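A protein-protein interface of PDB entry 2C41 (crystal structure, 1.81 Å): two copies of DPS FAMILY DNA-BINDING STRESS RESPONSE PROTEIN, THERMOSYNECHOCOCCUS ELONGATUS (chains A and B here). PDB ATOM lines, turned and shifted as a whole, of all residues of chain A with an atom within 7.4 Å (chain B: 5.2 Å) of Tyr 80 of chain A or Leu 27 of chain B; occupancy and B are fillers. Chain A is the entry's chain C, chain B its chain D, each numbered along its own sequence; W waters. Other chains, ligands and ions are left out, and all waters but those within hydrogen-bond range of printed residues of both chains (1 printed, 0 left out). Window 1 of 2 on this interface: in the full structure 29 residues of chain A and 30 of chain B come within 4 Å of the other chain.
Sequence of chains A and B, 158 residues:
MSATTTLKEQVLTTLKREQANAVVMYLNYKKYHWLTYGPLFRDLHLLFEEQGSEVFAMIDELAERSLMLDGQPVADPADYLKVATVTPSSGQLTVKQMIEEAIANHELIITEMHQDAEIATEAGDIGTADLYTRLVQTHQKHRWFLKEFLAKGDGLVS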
ATOM      1  N   LYS A  16       5.445 -16.694  15.191  1.00  0.00           N
ATOM      2  CA  LYS A  16       5.737 -17.914  15.947  1.00  0.00           C
ATOM      3  C   LYS A  16       6.780 -18.764  15.222  1.00  0.00           C
ATOM      4  O   LYS A  16       7.742 -19.239  15.839  1.00  0.00           O
ATOM      5  CB  LYS A  16       4.458 -18.718  16.211  1.00  0.00           C
ATOM      6  CG  LYS A  16       3.500 -18.037  17.172  1.00  0.00           C
ATOM      7  CD  LYS A  16       2.679 -19.085  17.911  1.00  0.00           C
ATOM      8  CE  LYS A  16       1.221 -18.705  18.105  1.00  0.00           C
ATOM      9  NZ  LYS A  16       0.886 -17.263  18.299  1.00  0.00           N
ATOM     10  N   ARG A  17       6.591 -18.945  13.915  1.00  0.00           N
ATOM     11  CA  ARG A  17       7.541 -19.698  13.099  1.00  0.00           C
ATOM     12  C   ARG A  17       8.919 -19.032  13.109  1.00  0.00           C
ATOM     13  O   ARG A  17       9.937 -19.703  13.302  1.00  0.00           O
ATOM     14  CB  ARG A  17       7.031 -19.843  11.658  1.00  0.00           C
ATOM     15  CG  ARG A  17       8.035 -20.518  10.704  1.00  0.00           C
ATOM     16  CD  ARG A  17       7.407 -20.887   9.337  1.00  0.00           C
ATOM     17  NE  ARG A  17       6.390 -19.929   8.890  1.00  0.00           N
ATOM     18  CZ  ARG A  17       6.634 -18.690   8.454  1.00  0.00           C
ATOM     19  NH1 ARG A  17       7.875 -18.220   8.398  1.00  0.00           N
ATOM     20  NH2 ARG A  17       5.619 -17.914   8.075  1.00  0.00           N
ATOM     21  N   GLN A  19      10.130 -16.851  15.290  1.00  0.00           N
ATOM     22  CA  GLN A  19      10.697 -16.904  16.643  1.00  0.00           C
ATOM     23  C   GLN A  19      11.313 -18.277  16.906  1.00  0.00           C
ATOM     24  O   GLN A  19      12.440 -18.375  17.382  1.00  0.00           O
ATOM     25  CB  GLN A  19       9.628 -16.618  17.695  1.00  0.00           C
ATOM     26  CG  GLN A  19      10.142 -16.772  19.131  1.00  0.00           C
ATOM     27  CD  GLN A  19       9.048 -17.095  20.123  1.00  0.00           C
ATOM     28  OE1 GLN A  19       9.324 -17.532  21.243  1.00  0.00           O
ATOM     29  NE2 GLN A  19       7.807 -16.890  19.725  1.00  0.00           N
ATOM     30  N   ALA A  20      10.557 -19.326  16.585  1.00  0.00           N
ATOM     31  CA  ALA A  20      11.028 -20.705  16.734  1.00  0.00           C
ATOM     32  C   ALA A  20      12.305 -20.941  15.929  1.00  0.00           C
ATOM     33  O   ALA A  20      13.241 -21.562  16.435  1.00  0.00           O
ATOM     34  CB  ALA A  20       9.925 -21.706  16.313  1.00  0.00           C
ATOM     35  N   ASN A  21      12.342 -20.420  14.697  1.00  0.00           N
ATOM     36  CA  ASN A  21      13.537 -20.501  13.852  1.00  0.00           C
ATOM     37  C   ASN A  21      14.747 -19.813  14.479  1.00  0.00           C
ATOM     38  O   ASN A  21      15.862 -20.323  14.395  1.00  0.00           O
ATOM     39  CB  ASN A  21      13.291 -19.945  12.443  1.00  0.00           C
ATOM     40  CG  ASN A  21      12.458 -20.880  11.574  1.00  0.00           C
ATOM     41  OD1 ASN A  21      11.956 -20.479  10.517  1.00  0.00           O
ATOM     42  ND2 ASN A  21      12.314 -22.122  12.003  1.00  0.00           N
ATOM     43  N   ALA A  22      14.522 -18.664  15.115  1.00  0.00           N
ATOM     44  CA  ALA A  22      15.610 -17.944  15.785  1.00  0.00           C
ATOM     45  C   ALA A  22      16.197 -18.789  16.922  1.00  0.00           C
ATOM     46  O   ALA A  22      17.421 -18.857  17.096  1.00  0.00           O
ATOM     47  CB  ALA A  22      15.126 -16.604  16.303  1.00  0.00           C
ATOM     48  N   VAL A  23      15.323 -19.437  17.689  1.00  0.00           N
ATOM     49  CA  VAL A  23      15.757 -20.300  18.797  1.00  0.00           C
ATOM     50  C   VAL A  23      16.594 -21.481  18.282  1.00  0.00           C
ATOM     51  O   VAL A  23      17.685 -21.739  18.793  1.00  0.00           O
ATOM     52  CB  VAL A  23      14.549 -20.810  19.622  1.00  0.00           C
ATOM     53  CG1 VAL A  23      14.983 -21.894  20.618  1.00  0.00           C
ATOM     54  CG2 VAL A  23      13.872 -19.630  20.339  1.00  0.00           C
ATOM     55  N   VAL A  24      16.089 -22.190  17.267  1.00  0.00           N
ATOM     56  CA  VAL A  24      16.815 -23.346  16.714  1.00  0.00           C
ATOM     57  C   VAL A  24      18.121 -22.916  16.045  1.00  0.00           C
ATOM     58  O   VAL A  24      19.159 -23.564  16.215  1.00  0.00           O
ATOM     59  CB  VAL A  24      15.932 -24.172  15.733  1.00  0.00           C
ATOM     60  CG1 VAL A  24      16.745 -25.282  15.023  1.00  0.00           C
ATOM     61  CG2 VAL A  24      14.767 -24.758  16.487  1.00  0.00           C
ATOM     62  N   TYR A  26      19.883 -20.284  16.752  1.00  0.00           N
ATOM     63  CA  TYR A  26      20.796 -19.947  17.838  1.00  0.00           C
ATOM     64  C   TYR A  26      21.456 -21.202  18.419  1.00  0.00           C
ATOM     65  O   TYR A  26      22.683 -21.264  18.558  1.00  0.00           O
ATOM     66  CB  TYR A  26      20.078 -19.159  18.943  1.00  0.00           C
ATOM     67  CG  TYR A  26      20.965 -19.007  20.148  1.00  0.00           C
ATOM     68  CD1 TYR A  26      22.095 -18.191  20.090  1.00  0.00           C
ATOM     69  CD2 TYR A  26      20.715 -19.717  21.320  1.00  0.00           C
ATOM     70  CE1 TYR A  26      22.940 -18.049  21.183  1.00  0.00           C
ATOM     71  CE2 TYR A  26      21.570 -19.589  22.427  1.00  0.00           C
ATOM     72  CZ  TYR A  26      22.672 -18.750  22.334  1.00  0.00           C
ATOM     73  OH  TYR A  26      23.530 -18.591  23.395  1.00  0.00           O
ATOM     74  N   LEU A  27      20.640 -22.195  18.760  1.00  0.00           N
ATOM     75  CA  LEU A  27      21.154 -23.432  19.342  1.00  0.00           C
ATOM     76  C   LEU A  27      22.076 -24.177  18.368  1.00  0.00           C
ATOM     77  O   LEU A  27      23.082 -24.751  18.791  1.00  0.00           O
ATOM     78  CB  LEU A  27      20.017 -24.321  19.846  1.00  0.00           C
ATOM     79  CG  LEU A  27      19.213 -23.762  21.031  1.00  0.00           C
ATOM     80  CD1 LEU A  27      17.998 -24.634  21.293  1.00  0.00           C
ATOM     81  CD2 LEU A  27      20.082 -23.622  22.286  1.00  0.00           C
ATOM     82  N   ILE A  59      15.409 -13.497  19.127  1.00  0.00           N
ATOM     83  CA  ILE A  59      14.424 -14.322  19.816  1.00  0.00           C
ATOM     84  C   ILE A  59      13.435 -13.453  20.590  1.00  0.00           C
ATOM     85  O   ILE A  59      12.222 -13.568  20.413  1.00  0.00           O
ATOM     86  CB  ILE A  59      15.081 -15.352  20.772  1.00  0.00           C
ATOM     87  CG1 ILE A  59      15.969 -16.326  19.982  1.00  0.00           C
ATOM     88  CG2 ILE A  59      14.004 -16.091  21.561  1.00  0.00           C
ATOM     89  CD1 ILE A  59      16.953 -17.095  20.836  1.00  0.00           C
ATOM     90  N   ALA A  63       9.502 -12.703  19.710  1.00  0.00           N
ATOM     91  CA  ALA A  63       8.557 -13.157  20.722  1.00  0.00           C
ATOM     92  C   ALA A  63       7.694 -12.009  21.219  1.00  0.00           C
ATOM     93  O   ALA A  63       6.470 -12.108  21.248  1.00  0.00           O
ATOM     94  CB  ALA A  63       9.293 -13.811  21.881  1.00  0.00           C
ATOM     95  N   PRO A  73       3.600 -15.489  22.035  1.00  0.00           N
ATOM     96  CA  PRO A  73       4.705 -16.120  21.328  1.00  0.00           C
ATOM     97  C   PRO A  73       4.711 -17.628  21.576  1.00  0.00           C
ATOM     98  O   PRO A  73       3.942 -18.124  22.397  1.00  0.00           O
ATOM     99  CB  PRO A  73       5.933 -15.491  21.988  1.00  0.00           C
ATOM    100  CG  PRO A  73       5.495 -15.247  23.399  1.00  0.00           C
ATOM    101  CD  PRO A  73       4.035 -14.880  23.309  1.00  0.00           C
ATOM    102  N   VAL A  74       5.567 -18.352  20.862  1.00  0.00           N
ATOM    103  CA  VAL A  74       5.893 -19.713  21.258  1.00  0.00           C
ATOM    104  C   VAL A  74       6.574 -19.561  22.619  1.00  0.00           C
ATOM    105  O   VAL A  74       7.344 -18.617  22.823  1.00  0.00           O
ATOM    106  CB  VAL A  74       6.838 -20.396  20.251  1.00  0.00           C
ATOM    107  CG1 VAL A  74       7.113 -21.835  20.667  1.00  0.00           C
ATOM    108  CG2 VAL A  74       6.227 -20.360  18.832  1.00  0.00           C
ATOM    109  N   ALA A  75       6.281 -20.460  23.556  1.00  0.00           N
ATOM    110  CA  ALA A  75       6.853 -20.336  24.906  1.00  0.00           C
ATOM    111  C   ALA A  75       7.189 -21.671  25.573  1.00  0.00           C
ATOM    112  O   ALA A  75       8.191 -21.783  26.274  1.00  0.00           O
ATOM    113  CB  ALA A  75       5.926 -19.514  25.793  1.00  0.00           C
ATOM    114  N   ASP A  76       6.350 -22.684  25.361  1.00  0.00           N
ATOM    115  CA  ASP A  76       6.649 -24.019  25.892  1.00  0.00           C
ATOM    116  C   ASP A  76       7.870 -24.580  25.157  1.00  0.00           C
ATOM    117  O   ASP A  76       7.846 -24.689  23.939  1.00  0.00           O
ATOM    118  CB  ASP A  76       5.461 -24.977  25.706  1.00  0.00           C
ATOM    119  CG  ASP A  76       4.205 -24.543  26.461  1.00  0.00           C
ATOM    120  OD1 ASP A  76       3.196 -25.295  26.383  1.00  0.00           O
ATOM    121  OD2 ASP A  76       4.190 -23.474  27.119  1.00  0.00           O
ATOM    122  N   PRO A  77       8.951 -24.919  25.885  1.00  0.00           N
ATOM    123  CA  PRO A  77      10.132 -25.463  25.202  1.00  0.00           C
ATOM    124  C   PRO A  77       9.859 -26.624  24.238  1.00  0.00           C
ATOM    125  O   PRO A  77      10.522 -26.719  23.203  1.00  0.00           O
ATOM    126  CB  PRO A  77      11.008 -25.933  26.362  1.00  0.00           C
ATOM    127  CG  PRO A  77      10.689 -24.956  27.442  1.00  0.00           C
ATOM    128  CD  PRO A  77       9.192 -24.785  27.335  1.00  0.00           C
ATOM    129  N   ALA A  78       8.898 -27.490  24.568  1.00  0.00           N
ATOM    130  CA  ALA A  78       8.564 -28.614  23.688  1.00  0.00           C
ATOM    131  C   ALA A  78       7.959 -28.179  22.341  1.00  0.00           C
ATOM    132  O   ALA A  78       7.931 -28.973  21.391  1.00  0.00           O
ATOM    133  CB  ALA A  78       7.654 -29.623  24.396  1.00  0.00           C
ATOM    134  N   ASP A  79       7.483 -26.934  22.259  1.00  0.00           N
ATOM    135  CA  ASP A  79       6.850 -26.433  21.038  1.00  0.00           C
ATOM    136  C   ASP A  79       7.838 -25.985  19.954  1.00  0.00           C
ATOM    137  O   ASP A  79       7.489 -25.985  18.776  1.00  0.00           O
ATOM    138  CB  ASP A  79       5.861 -25.297  21.344  1.00  0.00           C
ATOM    139  CG  ASP A  79       4.571 -25.783  22.006  1.00  0.00           C
ATOM    140  OD1 ASP A  79       3.740 -24.929  22.386  1.00  0.00           O
ATOM    141  OD2 ASP A  79       4.371 -27.005  22.135  1.00  0.00           O
ATOM    142  N   TYR A  80       9.054 -25.604  20.340  1.00  0.00           N
ATOM    143  CA  TYR A  80       9.982 -24.983  19.384  1.00  0.00           C
ATOM    144  C   TYR A  80      10.261 -25.846  18.159  1.00  0.00           C
ATOM    145  O   TYR A  80      10.164 -25.372  17.033  1.00  0.00           O
ATOM    146  CB  TYR A  80      11.285 -24.563  20.057  1.00  0.00           C
ATOM    147  CG  TYR A  80      11.131 -23.320  20.910  1.00  0.00           C
ATOM    148  CD1 TYR A  80      10.811 -22.091  20.329  1.00  0.00           C
ATOM    149  CD2 TYR A  80      11.318 -23.374  22.296  1.00  0.00           C
ATOM    150  CE1 TYR A  80      10.659 -20.936  21.110  1.00  0.00           C
ATOM    151  CE2 TYR A  80      11.172 -22.230  23.085  1.00  0.00           C
ATOM    152  CZ  TYR A  80      10.853 -21.015  22.480  1.00  0.00           C
ATOM    153  OH  TYR A  80      10.722 -19.883  23.253  1.00  0.00           O
ATOM    154  N   LEU A  81      10.577 -27.115  18.386  1.00  0.00           N
ATOM    155  CA  LEU A  81      10.891 -28.020  17.283  1.00  0.00           C
ATOM    156  C   LEU A  81       9.657 -28.439  16.471  1.00  0.00           C
ATOM    157  O   LEU A  81       9.787 -28.952  15.357  1.00  0.00           O
ATOM    158  CB  LEU A  81      11.658 -29.237  17.796  1.00  0.00           C
ATOM    159  CG  LEU A  81      13.072 -28.945  18.312  1.00  0.00           C
ATOM    160  CD1 LEU A  81      13.744 -30.222  18.745  1.00  0.00           C
ATOM    161  CD2 LEU A  81      13.918 -28.255  17.262  1.00  0.00           C
ATOM    162  N   LYS A  82       8.472 -28.206  17.032  1.00  0.00           N
ATOM    163  CA  LYS A  82       7.214 -28.476  16.337  1.00  0.00           C
ATOM    164  C   LYS A  82       6.840 -27.360  15.372  1.00  0.00           C
ATOM    165  O   LYS A  82       6.115 -27.595  14.401  1.00  0.00           O
ATOM    166  CB  LYS A  82       6.073 -28.670  17.337  1.00  0.00           C
ATOM    167  CG  LYS A  82       6.224 -29.879  18.231  1.00  0.00           C
ATOM    168  CD  LYS A  82       4.953 -30.095  19.036  1.00  0.00           C
ATOM    169  CE  LYS A  82       5.024 -31.380  19.849  1.00  0.00           C
ATOM    170  NZ  LYS A  82       5.937 -31.244  21.019  1.00  0.00           N
ATOM    171  N   VAL A  83       7.342 -26.156  15.642  1.00  0.00           N
ATOM    172  CA  VAL A  83       6.939 -24.947  14.934  1.00  0.00           C
ATOM    173  C   VAL A  83       8.042 -24.491  13.962  1.00  0.00           C
ATOM    174  O   VAL A  83       7.754 -23.949  12.892  1.00  0.00           O
ATOM    175  CB  VAL A  83       6.577 -23.834  15.969  1.00  0.00           C
ATOM    176  CG1 VAL A  83       6.304 -22.496  15.300  1.00  0.00           C
ATOM    177  CG2 VAL A  83       5.368 -24.258  16.808  1.00  0.00           C
ATOM    178  N   ALA A  84       9.303 -24.731  14.338  1.00  0.00           N
ATOM    179  CA  ALA A  84      10.442 -24.320  13.518  1.00  0.00           C
ATOM    180  C   ALA A  84      10.445 -25.015  12.166  1.00  0.00           C
ATOM    181  O   ALA A  84      10.086 -26.192  12.057  1.00  0.00           O
ATOM    182  CB  ALA A  84      11.770 -24.588  14.244  1.00  0.00           C
ATOM    183  N   THR A  85      10.845 -24.274  11.140  1.00  0.00           N
ATOM    184  CA  THR A  85      11.045 -24.833   9.808  1.00  0.00           C
ATOM    185  C   THR A  85      12.522 -24.984   9.437  1.00  0.00           C
ATOM    186  O   THR A  85      12.838 -25.716   8.506  1.00  0.00           O
ATOM    187  CB  THR A  85      10.330 -24.011   8.730  1.00  0.00           C
ATOM    188  OG1 THR A  85      10.714 -22.636   8.851  1.00  0.00           O
ATOM    189  CG2 THR A  85       8.816 -24.139   8.883  1.00  0.00           C
ATOM    190  N   VAL A  86      13.418 -24.298  10.149  1.00  0.00           N
ATOM    191  CA  VAL A  86      14.855 -24.553   9.987  1.00  0.00           C
ATOM    192  C   VAL A  86      15.218 -25.946  10.513  1.00  0.00           C
ATOM    193  O   VAL A  86      14.556 -26.475  11.406  1.00  0.00           O
ATOM    194  CB  VAL A  86      15.765 -23.478  10.655  1.00  0.00           C
ATOM    195  CG1 VAL A  86      15.531 -22.124  10.024  1.00  0.00           C
ATOM    196  CG2 VAL A  86      15.532 -23.422  12.140  1.00  0.00           C
ATOM    197  N   ALA B  22      20.099 -26.239  32.101  1.00  0.00           N
ATOM    198  CA  ALA B  22      20.324 -24.799  31.939  1.00  0.00           C
ATOM    199  C   ALA B  22      19.535 -24.258  30.740  1.00  0.00           C
ATOM    200  O   ALA B  22      18.907 -23.196  30.832  1.00  0.00           O
ATOM    201  CB  ALA B  22      21.822 -24.492  31.762  1.00  0.00           C
ATOM    202  N   VAL B  23      19.577 -24.982  29.623  1.00  0.00           N
ATOM    203  CA  VAL B  23      18.854 -24.568  28.414  1.00  0.00           C
ATOM    204  C   VAL B  23      17.345 -24.547  28.657  1.00  0.00           C
ATOM    205  O   VAL B  23      16.676 -23.566  28.342  1.00  0.00           O
ATOM    206  CB  VAL B  23      19.216 -25.435  27.157  1.00  0.00           C
ATOM    207  CG1 VAL B  23      18.317 -25.099  25.966  1.00  0.00           C
ATOM    208  CG2 VAL B  23      20.690 -25.246  26.773  1.00  0.00           C
ATOM    209  N   VAL B  24      16.808 -25.624  29.221  1.00  0.00           N
ATOM    210  CA  VAL B  24      15.368 -25.709  29.455  1.00  0.00           C
ATOM    211  C   VAL B  24      14.929 -24.672  30.498  1.00  0.00           C
ATOM    212  O   VAL B  24      13.904 -24.013  30.343  1.00  0.00           O
ATOM    213  CB  VAL B  24      14.945 -27.146  29.862  1.00  0.00           C
ATOM    214  CG1 VAL B  24      13.462 -27.214  30.148  1.00  0.00           C
ATOM    215  CG2 VAL B  24      15.336 -28.126  28.753  1.00  0.00           C
ATOM    216  N   MET B  25      15.725 -24.518  31.551  1.00  0.00           N
ATOM    217  CA  MET B  25      15.427 -23.543  32.598  1.00  0.00           C
ATOM    218  C   MET B  25      15.414 -22.134  32.027  1.00  0.00           C
ATOM    219  O   MET B  25      14.553 -21.324  32.374  1.00  0.00           O
ATOM    220  CB  MET B  25      16.461 -23.650  33.719  1.00  0.00           C
ATOM    221  CG  MET B  25      16.034 -23.033  35.019  1.00  0.00           C
ATOM    222  SD  MET B  25      14.632 -23.915  35.740  1.00  0.00           S
ATOM    223  CE  MET B  25      14.352 -22.894  37.185  1.00  0.00           C
ATOM    224  N   TYR B  26      16.374 -21.848  31.150  1.00  0.00           N
ATOM    225  CA  TYR B  26      16.423 -20.561  30.475  1.00  0.00           C
ATOM    226  C   TYR B  26      15.164 -20.320  29.637  1.00  0.00           C
ATOM    227  O   TYR B  26      14.530 -19.263  29.732  1.00  0.00           O
ATOM    228  CB  TYR B  26      17.660 -20.452  29.584  1.00  0.00           C
ATOM    229  CG  TYR B  26      17.602 -19.213  28.750  1.00  0.00           C
ATOM    230  CD1 TYR B  26      17.700 -17.957  29.346  1.00  0.00           C
ATOM    231  CD2 TYR B  26      17.389 -19.287  27.380  1.00  0.00           C
ATOM    232  CE1 TYR B  26      17.627 -16.809  28.593  1.00  0.00           C
ATOM    233  CE2 TYR B  26      17.303 -18.137  26.615  1.00  0.00           C
ATOM    234  CZ  TYR B  26      17.428 -16.906  27.231  1.00  0.00           C
ATOM    235  OH  TYR B  26      17.350 -15.758  26.485  1.00  0.00           O
ATOM    236  N   LEU B  27      14.809 -21.300  28.806  1.00  0.00           N
ATOM    237  CA  LEU B  27      13.616 -21.169  27.963  1.00  0.00           C
ATOM    238  C   LEU B  27      12.343 -21.023  28.801  1.00  0.00           C
ATOM    239  O   LEU B  27      11.457 -20.255  28.440  1.00  0.00           O
ATOM    240  CB  LEU B  27      13.508 -22.328  26.973  1.00  0.00           C
ATOM    241  CG  LEU B  27      14.621 -22.365  25.911  1.00  0.00           C
ATOM    242  CD1 LEU B  27      14.617 -23.696  25.145  1.00  0.00           C
ATOM    243  CD2 LEU B  27      14.544 -21.179  24.952  1.00  0.00           C
ATOM    244  N   ASN B  28      12.259 -21.754  29.917  1.00  0.00           N
ATOM    245  CA  ASN B  28      11.177 -21.560  30.896  1.00  0.00           C
ATOM    246  C   ASN B  28      11.113 -20.104  31.380  1.00  0.00           C
ATOM    247  O   ASN B  28      10.032 -19.509  31.424  1.00  0.00           O
ATOM    248  CB  ASN B  28      11.339 -22.479  32.113  1.00  0.00           C
ATOM    249  CG  ASN B  28      10.918 -23.924  31.847  1.00  0.00           C
ATOM    250  OD1 ASN B  28      11.086 -24.800  32.719  1.00  0.00           O
ATOM    251  ND2 ASN B  28      10.399 -24.190  30.661  1.00  0.00           N
ATOM    252  N   TYR B  29      12.264 -19.540  31.750  1.00  0.00           N
ATOM    253  CA  TYR B  29      12.317 -18.139  32.191  1.00  0.00           C
ATOM    254  C   TYR B  29      11.833 -17.162  31.127  1.00  0.00           C
ATOM    255  O   TYR B  29      11.164 -16.170  31.441  1.00  0.00           O
ATOM    256  CB  TYR B  29      13.728 -17.741  32.635  1.00  0.00           C
ATOM    257  CG  TYR B  29      13.930 -17.846  34.130  1.00  0.00           C
ATOM    258  CD1 TYR B  29      13.104 -17.136  35.010  1.00  0.00           C
ATOM    259  CD2 TYR B  29      14.939 -18.660  34.672  1.00  0.00           C
ATOM    260  CE1 TYR B  29      13.274 -17.231  36.398  1.00  0.00           C
ATOM    261  CE2 TYR B  29      15.125 -18.749  36.060  1.00  0.00           C
ATOM    262  CZ  TYR B  29      14.285 -18.025  36.908  1.00  0.00           C
ATOM    263  OH  TYR B  29      14.449 -18.084  38.268  1.00  0.00           O
ATOM    264  N   LYS B  30      12.167 -17.440  29.871  1.00  0.00           N
ATOM    265  CA  LYS B  30      11.679 -16.599  28.777  1.00  0.00           C
ATOM    266  C   LYS B  30      10.165 -16.682  28.678  1.00  0.00           C
ATOM    267  O   LYS B  30       9.501 -15.653  28.512  1.00  0.00           O
ATOM    268  CB  LYS B  30      12.348 -16.938  27.442  1.00  0.00           C
ATOM    269  CG  LYS B  30      13.857 -16.652  27.400  1.00  0.00           C
ATOM    270  CD  LYS B  30      14.219 -15.185  27.734  1.00  0.00           C
ATOM    271  CE  LYS B  30      13.471 -14.146  26.878  1.00  0.00           C
ATOM    272  NZ  LYS B  30      14.157 -12.812  26.881  1.00  0.00           N
ATOM    273  N   LYS B  31       9.619 -17.893  28.816  1.00  0.00           N
ATOM    274  CA  LYS B  31       8.163 -18.051  28.878  1.00  0.00           C
ATOM    275  C   LYS B  31       7.556 -17.139  29.947  1.00  0.00           C
ATOM    276  O   LYS B  31       6.629 -16.381  29.662  1.00  0.00           O
ATOM    277  CB  LYS B  31       7.769 -19.507  29.146  1.00  0.00           C
ATOM    278  CG  LYS B  31       6.259 -19.694  29.385  1.00  0.00           C
ATOM    279  CD  LYS B  31       5.858 -21.157  29.452  1.00  0.00           C
ATOM    280  CE  LYS B  31       4.352 -21.331  29.632  1.00  0.00           C
ATOM    281  NZ  LYS B  31       4.004 -22.785  29.804  1.00  0.00           N
ATOM    282  N   TRP B  34       7.809 -13.431  29.068  1.00  0.00           N
ATOM    283  CA  TRP B  34       6.854 -13.024  28.040  1.00  0.00           C
ATOM    284  C   TRP B  34       5.398 -13.068  28.490  1.00  0.00           C
ATOM    285  O   TRP B  34       4.608 -12.197  28.096  1.00  0.00           O
ATOM    286  CB  TRP B  34       7.011 -13.875  26.765  1.00  0.00           C
ATOM    287  CG  TRP B  34       8.348 -13.751  26.108  1.00  0.00           C
ATOM    288  CD1 TRP B  34       9.119 -12.624  26.011  1.00  0.00           C
ATOM    289  CD2 TRP B  34       9.069 -14.791  25.436  1.00  0.00           C
ATOM    290  NE1 TRP B  34      10.288 -12.905  25.336  1.00  0.00           N
ATOM    291  CE2 TRP B  34      10.284 -14.227  24.976  1.00  0.00           C
ATOM    292  CE3 TRP B  34       8.819 -16.152  25.198  1.00  0.00           C
ATOM    293  CZ2 TRP B  34      11.241 -14.970  24.282  1.00  0.00           C
ATOM    294  CZ3 TRP B  34       9.777 -16.895  24.497  1.00  0.00           C
ATOM    295  CH2 TRP B  34      10.970 -16.301  24.053  1.00  0.00           C
HETATM  296  O   HOH W   1      10.520 -20.503  25.797  1.00  0.00           O
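Of the 11 printed residues of chain B, 4 touch a printed residue of chain A.
Hydrophobic or aromatic side chains of chain B that line the printed part of chain A: Leu 27 and Trp 34.
Along chain B the printed residues that touch a printed residue of chain A span positions 27 to 34.
Along chain A the printed residues that touch a printed residue of chain B span positions 19 to 80.
Among the printed residues, 11 pairs touch across the chains.
Among the printed residues, Asp or Glu carboxylates within 4 Å of a Lys or Arg side-chain nitrogen of the other chain: Asp 76 of chain A with Lys 31 of chain B.
Positions printed for both chains: 22, 23, 24, 26 and 27.
Of the 11 pairs that touch across the chains among the printed residues, none has its exchanged pair printed and touching as well.
OE1 of Gln 19 of chain A lies close to O of Val 74 of chain A (2.8 Å).
The side-chain hydroxyl (OH) of Tyr 80 of chain A sits at hydrogen-bond distance from the side-chain amide oxygen (OE1) of Gln 19 of chain A (3.4 Å).
The side-chain carboxylate (OD2) of Asp 76 of chain A lies within salt-bridge range of the side-chain amino group (NZ) of Lys 31 of chain B (2.8 Å).
Among the printed residues, pairs that only touch across the chains: Ala 63 of chain A with Trp 34 of chain B, Pro 77 of chain A with Asn 28 of chain B, Gln 19 of chain A with Trp 34 of chain B, Tyr 80 of chain A with Trp 34 of chain B, Val 74 of chain A with Trp 34 of chain B, Ala 75 of chain A with Lys 31 of chain B, Pro 77 of chain A with Leu 27 of chain B, Pro 73 of chain A with Trp 34 of chain B, Ile 59 of chain A with Trp 34 of chain B and Tyr 80 of chain A with Leu 27 of chain B.
Printed residues of chain B within 4 Å of Tyr 80 of chain A: Leu 27 and Trp 34.
Printed residues of chain A within 4 Å of Leu 27 of chain B: Pro 77 and Tyr 80.
Printed residues of chain B within 4 Å of Ala 63 of chain A: Trp 34 (3.3 Å).
Printed residues of chain B within 4 Å of Ala 75 of chain A: Lys 31 (3.6 Å).
Printed residues of chain A within 4 Å of Trp 34 of chain B: Gln 19 (3.3 Å), Ile 59 (3.9 Å), Ala 63 (3.3 Å), Pro 73 (3.9 Å), Val 74 (3.4 Å) and Tyr 80 (3.4 Å).
Of the printed residues of chain B, Pro 77 of chain A touches Leu 27 and Asn 28.
Ala 22 of chain B touches none of the printed residues of chain A.
Ala 78 of chain A touches none of the printed residues of chain B.
The nearest printed residue of chain B that does not touch Tyr 80 of chain A is Lys 30 of chain B (5.4 Å).
The nearest printed residue of chain A that does not touch Leu 27 of chain B is Ala 75 of chain A (4.2 Å).
Water W1 lies within hydrogen-bond range of the side-chain hydroxyl (OH) of Tyr 80 of chain A (2.6 Å), the backbone carbonyl oxygen (O) of Ala 75 of chain A (2.7 Å) and the backbone carbonyl oxygen (O) of Leu 27 of chain B (2.8 Å).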
